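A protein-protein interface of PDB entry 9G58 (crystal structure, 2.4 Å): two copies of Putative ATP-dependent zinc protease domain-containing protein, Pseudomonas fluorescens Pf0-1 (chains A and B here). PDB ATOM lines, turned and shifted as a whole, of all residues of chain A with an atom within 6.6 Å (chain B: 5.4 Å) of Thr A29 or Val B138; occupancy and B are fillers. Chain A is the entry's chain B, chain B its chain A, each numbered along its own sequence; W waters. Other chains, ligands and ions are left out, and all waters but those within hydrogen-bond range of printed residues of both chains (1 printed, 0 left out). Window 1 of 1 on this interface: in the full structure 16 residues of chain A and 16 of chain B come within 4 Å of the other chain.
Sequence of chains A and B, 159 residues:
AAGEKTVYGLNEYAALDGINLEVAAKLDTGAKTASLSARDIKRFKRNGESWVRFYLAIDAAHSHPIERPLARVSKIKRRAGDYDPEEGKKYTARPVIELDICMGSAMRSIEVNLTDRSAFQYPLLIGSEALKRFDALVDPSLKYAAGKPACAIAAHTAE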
ATOM      1  N   LEU A  27      10.010 -18.900 -10.563  1.00  0.00           N
ATOM      2  CA  LEU A  27      11.031 -18.418  -9.638  1.00  0.00           C
ATOM      3  C   LEU A  27      11.978 -17.498 -10.408  1.00  0.00           C
ATOM      4  O   LEU A  27      12.746 -17.955 -11.262  1.00  0.00           O
ATOM      5  CB  LEU A  27      11.769 -19.588  -8.990  1.00  0.00           C
ATOM      6  CG  LEU A  27      11.053 -20.305  -7.834  1.00  0.00           C
ATOM      7  CD1 LEU A  27       9.803 -21.061  -8.286  1.00  0.00           C
ATOM      8  CD2 LEU A  27      12.004 -21.253  -7.136  1.00  0.00           C
ATOM      9  N   ASP A  28      11.898 -16.200 -10.128  1.00  0.00           N
ATOM     10  CA  ASP A  28      12.549 -15.158 -10.922  1.00  0.00           C
ATOM     11  C   ASP A  28      13.517 -14.390 -10.023  1.00  0.00           C
ATOM     12  O   ASP A  28      13.104 -13.501  -9.273  1.00  0.00           O
ATOM     13  CB  ASP A  28      11.495 -14.243 -11.541  1.00  0.00           C
ATOM     14  CG  ASP A  28      12.080 -13.211 -12.482  1.00  0.00           C
ATOM     15  OD1 ASP A  28      13.322 -13.130 -12.605  1.00  0.00           O
ATOM     16  OD2 ASP A  28      11.283 -12.481 -13.111  1.00  0.00           O
ATOM     17  N   THR A  29      14.811 -14.716 -10.110  1.00  0.00           N
ATOM     18  CA  THR A  29      15.807 -14.006  -9.314  1.00  0.00           C
ATOM     19  C   THR A  29      16.088 -12.600  -9.830  1.00  0.00           C
ATOM     20  O   THR A  29      16.679 -11.800  -9.096  1.00  0.00           O
ATOM     21  CB  THR A  29      17.116 -14.797  -9.265  1.00  0.00           C
ATOM     22  OG1 THR A  29      17.645 -14.934 -10.590  1.00  0.00           O
ATOM     23  CG2 THR A  29      16.886 -16.173  -8.657  1.00  0.00           C
ATOM     24  N   GLY A  30      15.665 -12.274 -11.051  1.00  0.00           N
ATOM     25  CA  GLY A  30      15.846 -10.939 -11.588  1.00  0.00           C
ATOM     26  C   GLY A  30      14.861  -9.908 -11.084  1.00  0.00           C
ATOM     27  O   GLY A  30      15.071  -8.710 -11.299  1.00  0.00           O
ATOM     28  N   ALA A  31      13.786 -10.342 -10.438  1.00  0.00           N
ATOM     29  CA  ALA A  31      12.811  -9.450  -9.831  1.00  0.00           C
ATOM     30  C   ALA A  31      12.958  -9.515  -8.316  1.00  0.00           C
ATOM     31  O   ALA A  31      13.175 -10.591  -7.753  1.00  0.00           O
ATOM     32  CB  ALA A  31      11.385  -9.825 -10.244  1.00  0.00           C
ATOM     33  N   LYS A  32      12.851  -8.359  -7.658  1.00  0.00           N
ATOM     34  CA  LYS A  32      12.986  -8.336  -6.205  1.00  0.00           C
ATOM     35  C   LYS A  32      11.688  -8.752  -5.527  1.00  0.00           C
ATOM     36  O   LYS A  32      11.688  -9.609  -4.637  1.00  0.00           O
ATOM     37  CB  LYS A  32      13.403  -6.942  -5.732  1.00  0.00           C
ATOM     38  CG  LYS A  32      14.761  -6.492  -6.231  1.00  0.00           C
ATOM     39  CD  LYS A  32      15.126  -5.130  -5.664  1.00  0.00           C
ATOM     40  CE  LYS A  32      16.173  -4.445  -6.523  1.00  0.00           C
ATOM     41  NZ  LYS A  32      17.357  -5.320  -6.725  1.00  0.00           N
ATOM     42  N   ILE A 126       7.648 -15.368  -8.158  1.00  0.00           N
ATOM     43  CA  ILE A 126       8.390 -15.359  -6.903  1.00  0.00           C
ATOM     44  C   ILE A 126       9.729 -14.677  -7.145  1.00  0.00           C
ATOM     45  O   ILE A 126      10.608 -15.227  -7.818  1.00  0.00           O
ATOM     46  CB  ILE A 126       8.573 -16.775  -6.351  1.00  0.00           C
ATOM     47  CG1 ILE A 126       7.204 -17.419  -6.137  1.00  0.00           C
ATOM     48  CG2 ILE A 126       9.373 -16.741  -5.056  1.00  0.00           C
ATOM     49  CD1 ILE A 126       7.266 -18.728  -5.442  1.00  0.00           C
ATOM     50  N   GLY A 127       9.894 -13.486  -6.577  1.00  0.00           N
ATOM     51  CA  GLY A 127      11.087 -12.695  -6.773  1.00  0.00           C
ATOM     52  C   GLY A 127      12.212 -13.096  -5.838  1.00  0.00           C
ATOM     53  O   GLY A 127      12.144 -14.084  -5.106  1.00  0.00           O
ATOM     54  N   SER A 128      13.286 -12.302  -5.886  1.00  0.00           N
ATOM     55  CA  SER A 128      14.490 -12.639  -5.131  1.00  0.00           C
ATOM     56  C   SER A 128      14.261 -12.534  -3.626  1.00  0.00           C
ATOM     57  O   SER A 128      14.788 -13.347  -2.859  1.00  0.00           O
ATOM     58  CB  SER A 128      15.651 -11.745  -5.571  1.00  0.00           C
ATOM     59  OG  SER A 128      15.370 -10.376  -5.347  1.00  0.00           O
ATOM     60  N   LEU A 131      12.334 -15.550  -2.484  1.00  0.00           N
ATOM     61  CA  LEU A 131      13.246 -16.687  -2.555  1.00  0.00           C
ATOM     62  C   LEU A 131      14.245 -16.679  -1.406  1.00  0.00           C
ATOM     63  O   LEU A 131      14.640 -17.748  -0.925  1.00  0.00           O
ATOM     64  CB  LEU A 131      13.967 -16.694  -3.902  1.00  0.00           C
ATOM     65  CG  LEU A 131      13.090 -17.018  -5.114  1.00  0.00           C
ATOM     66  CD1 LEU A 131      13.806 -16.714  -6.418  1.00  0.00           C
ATOM     67  CD2 LEU A 131      12.669 -18.471  -5.068  1.00  0.00           C
ATOM     68  N   ALA A 136      16.012 -20.484  -0.582  1.00  0.00           N
ATOM     69  CA  ALA A 136      15.991 -21.220  -1.834  1.00  0.00           C
ATOM     70  C   ALA A 136      17.287 -21.027  -2.612  1.00  0.00           C
ATOM     71  O   ALA A 136      17.913 -19.967  -2.568  1.00  0.00           O
ATOM     72  CB  ALA A 136      14.809 -20.782  -2.702  1.00  0.00           C
ATOM     73  N   LEU A 137      17.682 -22.084  -3.315  1.00  0.00           N
ATOM     74  CA  LEU A 137      18.683 -22.034  -4.369  1.00  0.00           C
ATOM     75  C   LEU A 137      17.985 -22.415  -5.662  1.00  0.00           C
ATOM     76  O   LEU A 137      17.360 -23.478  -5.739  1.00  0.00           O
ATOM     77  CB  LEU A 137      19.847 -22.992  -4.108  1.00  0.00           C
ATOM     78  CG  LEU A 137      20.582 -22.956  -2.773  1.00  0.00           C
ATOM     79  CD1 LEU A 137      21.706 -23.980  -2.774  1.00  0.00           C
ATOM     80  CD2 LEU A 137      21.128 -21.569  -2.508  1.00  0.00           C
ATOM     81  N   VAL A 138      18.090 -21.564  -6.673  1.00  0.00           N
ATOM     82  CA  VAL A 138      17.377 -21.782  -7.924  1.00  0.00           C
ATOM     83  C   VAL A 138      18.296 -22.510  -8.897  1.00  0.00           C
ATOM     84  O   VAL A 138      19.337 -21.981  -9.300  1.00  0.00           O
ATOM     85  CB  VAL A 138      16.874 -20.458  -8.517  1.00  0.00           C
ATOM     86  CG1 VAL A 138      16.132 -20.717  -9.818  1.00  0.00           C
ATOM     87  CG2 VAL A 138      15.972 -19.747  -7.521  1.00  0.00           C
ATOM     88  N   ASP A 139      17.911 -23.733  -9.264  1.00  0.00           N
ATOM     89  CA  ASP A 139      18.597 -24.493 -10.297  1.00  0.00           C
ATOM     90  C   ASP A 139      17.869 -24.247 -11.607  1.00  0.00           C
ATOM     91  O   ASP A 139      16.741 -24.735 -11.778  1.00  0.00           O
ATOM     92  CB  ASP A 139      18.602 -25.978  -9.962  1.00  0.00           C
ATOM     93  CG  ASP A 139      19.525 -26.781 -10.866  1.00  0.00           C
ATOM     94  OD1 ASP A 139      19.780 -26.351 -12.009  1.00  0.00           O
ATOM     95  OD2 ASP A 139      19.990 -27.856 -10.433  1.00  0.00           O
ATOM     96  N   PRO A 140      18.452 -23.501 -12.551  1.00  0.00           N
ATOM     97  CA  PRO A 140      17.758 -23.241 -13.820  1.00  0.00           C
ATOM     98  C   PRO A 140      17.585 -24.474 -14.691  1.00  0.00           C
ATOM     99  O   PRO A 140      16.790 -24.428 -15.638  1.00  0.00           O
ATOM    100  CB  PRO A 140      18.660 -22.205 -14.506  1.00  0.00           C
ATOM    101  CG  PRO A 140      20.005 -22.439 -13.914  1.00  0.00           C
ATOM    102  CD  PRO A 140      19.759 -22.828 -12.488  1.00  0.00           C
ATOM    103  N   TYR B   8      26.294 -19.489  -7.075  1.00  0.00           N
ATOM    104  CA  TYR B   8      26.557 -18.071  -7.274  1.00  0.00           C
ATOM    105  C   TYR B   8      25.410 -17.282  -6.657  1.00  0.00           C
ATOM    106  O   TYR B   8      24.406 -17.854  -6.233  1.00  0.00           O
ATOM    107  CB  TYR B   8      26.702 -17.730  -8.763  1.00  0.00           C
ATOM    108  CG  TYR B   8      27.779 -18.493  -9.500  1.00  0.00           C
ATOM    109  CD1 TYR B   8      29.102 -18.070  -9.475  1.00  0.00           C
ATOM    110  CD2 TYR B   8      27.471 -19.633 -10.229  1.00  0.00           C
ATOM    111  CE1 TYR B   8      30.087 -18.767 -10.155  1.00  0.00           C
ATOM    112  CE2 TYR B   8      28.445 -20.335 -10.909  1.00  0.00           C
ATOM    113  CZ  TYR B   8      29.751 -19.898 -10.871  1.00  0.00           C
ATOM    114  OH  TYR B   8      30.719 -20.602 -11.551  1.00  0.00           O
ATOM    115  N   GLY B   9      25.544 -15.953  -6.633  1.00  0.00           N
ATOM    116  CA  GLY B   9      24.560 -15.080  -6.041  1.00  0.00           C
ATOM    117  C   GLY B   9      23.751 -14.314  -7.073  1.00  0.00           C
ATOM    118  O   GLY B   9      23.839 -14.551  -8.279  1.00  0.00           O
ATOM    119  N   LEU B  10      22.936 -13.378  -6.571  1.00  0.00           N
ATOM    120  CA  LEU B  10      22.155 -12.524  -7.465  1.00  0.00           C
ATOM    121  C   LEU B  10      23.048 -11.708  -8.386  1.00  0.00           C
ATOM    122  O   LEU B  10      22.673 -11.433  -9.532  1.00  0.00           O
ATOM    123  CB  LEU B  10      21.253 -11.580  -6.673  1.00  0.00           C
ATOM    124  CG  LEU B  10      20.042 -12.168  -5.955  1.00  0.00           C
ATOM    125  CD1 LEU B  10      19.290 -11.086  -5.193  1.00  0.00           C
ATOM    126  CD2 LEU B  10      19.127 -12.867  -6.954  1.00  0.00           C
ATOM    127  N   LYS B  26      24.123  -9.540 -13.407  1.00  0.00           N
ATOM    128  CA  LYS B  26      22.921  -9.858 -12.654  1.00  0.00           C
ATOM    129  C   LYS B  26      22.447 -11.234 -13.099  1.00  0.00           C
ATOM    130  O   LYS B  26      22.146 -11.438 -14.279  1.00  0.00           O
ATOM    131  CB  LYS B  26      21.844  -8.799 -12.887  1.00  0.00           C
ATOM    132  CG  LYS B  26      20.513  -9.091 -12.228  1.00  0.00           C
ATOM    133  CD  LYS B  26      19.507  -8.001 -12.553  1.00  0.00           C
ATOM    134  CE  LYS B  26      18.335  -8.028 -11.588  1.00  0.00           C
ATOM    135  NZ  LYS B  26      17.293  -7.030 -11.958  1.00  0.00           N
ATOM    136  N   LEU B  27      22.385 -12.174 -12.161  1.00  0.00           N
ATOM    137  CA  LEU B  27      21.990 -13.545 -12.465  1.00  0.00           C
ATOM    138  C   LEU B  27      20.471 -13.621 -12.389  1.00  0.00           C
ATOM    139  O   LEU B  27      19.891 -13.574 -11.299  1.00  0.00           O
ATOM    140  CB  LEU B  27      22.660 -14.530 -11.513  1.00  0.00           C
ATOM    141  CG  LEU B  27      24.123 -14.879 -11.815  1.00  0.00           C
ATOM    142  CD1 LEU B  27      25.070 -13.700 -11.599  1.00  0.00           C
ATOM    143  CD2 LEU B  27      24.559 -16.067 -10.985  1.00  0.00           C
ATOM    144  N   ASP B  28      19.833 -13.745 -13.550  1.00  0.00           N
ATOM    145  CA  ASP B  28      18.392 -13.574 -13.714  1.00  0.00           C
ATOM    146  C   ASP B  28      17.803 -14.886 -14.221  1.00  0.00           C
ATOM    147  O   ASP B  28      17.846 -15.170 -15.421  1.00  0.00           O
ATOM    148  CB  ASP B  28      18.114 -12.420 -14.678  1.00  0.00           C
ATOM    149  CG  ASP B  28      16.639 -12.105 -14.823  1.00  0.00           C
ATOM    150  OD1 ASP B  28      15.799 -12.823 -14.238  1.00  0.00           O
ATOM    151  OD2 ASP B  28      16.321 -11.131 -15.540  1.00  0.00           O
ATOM    152  N   THR B  29      17.235 -15.674 -13.306  1.00  0.00           N
ATOM    153  CA  THR B  29      16.592 -16.928 -13.681  1.00  0.00           C
ATOM    154  C   THR B  29      15.248 -16.717 -14.364  1.00  0.00           C
ATOM    155  O   THR B  29      14.698 -17.675 -14.914  1.00  0.00           O
ATOM    156  CB  THR B  29      16.415 -17.824 -12.455  1.00  0.00           C
ATOM    157  OG1 THR B  29      15.553 -17.182 -11.508  1.00  0.00           O
ATOM    158  CG2 THR B  29      17.762 -18.094 -11.800  1.00  0.00           C
ATOM    159  N   GLY B  30      14.693 -15.506 -14.315  1.00  0.00           N
ATOM    160  CA  GLY B  30      13.450 -15.217 -15.006  1.00  0.00           C
ATOM    161  C   GLY B  30      13.580 -14.947 -16.491  1.00  0.00           C
ATOM    162  O   GLY B  30      12.570 -14.953 -17.200  1.00  0.00           O
ATOM    163  N   LEU B 131      23.012 -19.666 -17.209  1.00  0.00           N
ATOM    164  CA  LEU B 131      23.201 -20.235 -15.877  1.00  0.00           C
ATOM    165  C   LEU B 131      23.233 -21.757 -15.932  1.00  0.00           C
ATOM    166  O   LEU B 131      23.966 -22.400 -15.172  1.00  0.00           O
ATOM    167  CB  LEU B 131      22.087 -19.759 -14.946  1.00  0.00           C
ATOM    168  CG  LEU B 131      22.060 -18.275 -14.587  1.00  0.00           C
ATOM    169  CD1 LEU B 131      20.748 -17.919 -13.899  1.00  0.00           C
ATOM    170  CD2 LEU B 131      23.245 -17.920 -13.714  1.00  0.00           C
ATOM    171  N   ALA B 136      25.021 -23.660 -12.685  1.00  0.00           N
ATOM    172  CA  ALA B 136      24.888 -22.704 -11.599  1.00  0.00           C
ATOM    173  C   ALA B 136      23.638 -22.959 -10.767  1.00  0.00           C
ATOM    174  O   ALA B 136      22.604 -23.406 -11.271  1.00  0.00           O
ATOM    175  CB  ALA B 136      24.860 -21.272 -12.139  1.00  0.00           C
ATOM    176  N   LEU B 137      23.762 -22.682  -9.474  1.00  0.00           N
ATOM    177  CA  LEU B 137      22.640 -22.541  -8.560  1.00  0.00           C
ATOM    178  C   LEU B 137      22.650 -21.111  -8.047  1.00  0.00           C
ATOM    179  O   LEU B 137      23.678 -20.633  -7.561  1.00  0.00           O
ATOM    180  CB  LEU B 137      22.735 -23.520  -7.388  1.00  0.00           C
ATOM    181  CG  LEU B 137      22.956 -24.999  -7.696  1.00  0.00           C
ATOM    182  CD1 LEU B 137      22.979 -25.814  -6.410  1.00  0.00           C
ATOM    183  CD2 LEU B 137      21.890 -25.512  -8.645  1.00  0.00           C
ATOM    184  N   VAL B 138      21.524 -20.422  -8.176  1.00  0.00           N
ATOM    185  CA  VAL B 138      21.436 -19.017  -7.798  1.00  0.00           C
ATOM    186  C   VAL B 138      20.895 -18.909  -6.377  1.00  0.00           C
ATOM    187  O   VAL B 138      19.755 -19.294  -6.103  1.00  0.00           O
ATOM    188  CB  VAL B 138      20.568 -18.227  -8.786  1.00  0.00           C
ATOM    189  CG1 VAL B 138      20.477 -16.774  -8.355  1.00  0.00           C
ATOM    190  CG2 VAL B 138      21.165 -18.319 -10.178  1.00  0.00           C
ATOM    191  N   ASP B 139      21.725 -18.384  -5.473  1.00  0.00           N
ATOM    192  CA  ASP B 139      21.331 -18.069  -4.112  1.00  0.00           C
ATOM    193  C   ASP B 139      20.952 -16.599  -4.052  1.00  0.00           C
ATOM    194  O   ASP B 139      21.838 -15.738  -4.160  1.00  0.00           O
ATOM    195  CB  ASP B 139      22.474 -18.365  -3.140  1.00  0.00           C
ATOM    196  CG  ASP B 139      22.038 -18.313  -1.684  1.00  0.00           C
ATOM    197  OD1 ASP B 139      21.061 -17.600  -1.366  1.00  0.00           O
ATOM    198  OD2 ASP B 139      22.677 -18.994  -0.854  1.00  0.00           O
ATOM    199  N   PRO B 140      19.671 -16.259  -3.900  1.00  0.00           N
ATOM    200  CA  PRO B 140      19.290 -14.842  -3.811  1.00  0.00           C
ATOM    201  C   PRO B 140      19.787 -14.145  -2.555  1.00  0.00           C
ATOM    202  O   PRO B 140      19.731 -12.909  -2.497  1.00  0.00           O
ATOM    203  CB  PRO B 140      17.758 -14.890  -3.854  1.00  0.00           C
ATOM    204  CG  PRO B 140      17.415 -16.259  -3.372  1.00  0.00           C
ATOM    205  CD  PRO B 140      18.502 -17.151  -3.879  1.00  0.00           C
HETATM  206  O   HOH W   1      12.220 -18.508 -14.046  1.00  0.00           O
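O of Thr A29 touches CD2 of Leu B10, at 3.4 Å.
CG2 of Thr A29 touches CG1 of Val B138, at 3.7 Å.
CB of Ser A128 touches CD1 of Leu B10, at 3.7 Å.
Pro B140 touches Leu A131.
Ala A136 touches Pro B140 (O to CD, 3.2 Å).
Val A138 touches Thr B29.
O of Val A138 touches CA of Leu B137 (3.4 Å).
Leu B137 touches Asp A139.
CB of Leu B131 touches CG of Pro A140, at 3.5 Å.
CD of Pro A140 touches O of Ala B136, 3.1 Å away.
Asp B28 touches its own counterpart, Asp A28.
Thr A29 touches Val B138, and with the chains exchanged Val A138 touches Thr B29.
Leu A137 touches Val B138, and with the chains exchanged Val A138 touches Leu B137.
Val A138 touches its own counterpart, Val B138.
10 positions are printed for both chains.
Of chain B, only Leu B10 (3.4 Å), Leu B27 (2.7 Å), Asp B28 (3.5 Å), Thr B29 (2.8 Å) and Val B138 (3.7 Å) come within 4 Å of Thr A29.
Of the printed residues of chain A, Leu B10 touches Thr A29 (3.4 Å) and Ser A128 (3.7 Å).
Of the printed residues of chain A, Asp B139 touches Leu A137.
The nearest residue of chain B that does not touch Thr A29 is Gly B30 (4.3 Å).
Of the 14 printed residues of chain B, 12 touch a printed residue of chain A.
Hydrophobic or aromatic side chains of chain B within 4 Å of the printed part of chain A: Leu B10, Leu B131, Leu B137, Val B138 and Pro B140.
Of the 15 printed residues of chain A, 11 touch a printed residue of chain B.
Hydrophobic or aromatic side chains of chain A within 4 Å of the printed part of chain B: Leu A131, Leu A137, Val A138 and Pro A140.
Among the printed residues, 23 pairs touch across the chains.
Among the printed residues, no Asp or Glu carboxylate lies within 4 Å of a Lys or Arg side-chain nitrogen of the other chain.
Water W1 lies within hydrogen-bond range of the backbone carbonyl oxygen of Thr B29 and the backbone carbonyl oxygen of Leu A27.
The backbone carbonyl oxygen (O) of Gly A30 lies within hydrogen-bond range of the side-chain amino group (NZ) of Lys B26.
The side-chain hydroxyl (OG1) of Thr A29 is in hydrogen-bond range of the backbone carbonyl oxygen (O) of Leu B27 (2.7 Å).
The backbone NH of Gly A30 sits at hydrogen-bond distance from the side-chain carboxylate of Asp B28.
The side-chain hydroxyl (OG1) of Thr B29 lies within hydrogen-bond range of the backbone carbonyl oxygen (O) of Leu A27 (2.9 Å).
N of Thr B29 lies within hydrogen-bond range of OG1 of Thr A29, 2.8 Å away.
The side-chain carboxylate of Asp A28 lies close to the backbone NH of Gly B30, at 3.2 Å.
The backbone carbonyl oxygen of Val B138 sits at hydrogen-bond distance from the backbone NH of Val A138 (2.9 Å).
The side-chain carboxylate (OD1) of Asp A28 lies close to the side-chain carboxylate (OD1) of Asp B28 (3.0 Å).
O of Leu B10 lies within hydrogen-bond range of N of Leu B27 (2.7 Å).
OD1 of Asp B28 sits at hydrogen-bond distance from N of Gly B30, 2.9 Å away.
The backbone NH (N) of Ala B136 is in hydrogen-bond range of the backbone carbonyl oxygen (O) of Leu B131, at 3.0 Å.
N of Gly A30 sits at hydrogen-bond distance from OD1 of Asp A28, 2.9 Å away.
The backbone NH of Ser A128 sits at hydrogen-bond distance from the backbone carbonyl oxygen of Ala A31 (2.5 Å).
O of Lys A32 lies within hydrogen-bond range of N of Ser A128 (3.4 Å).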
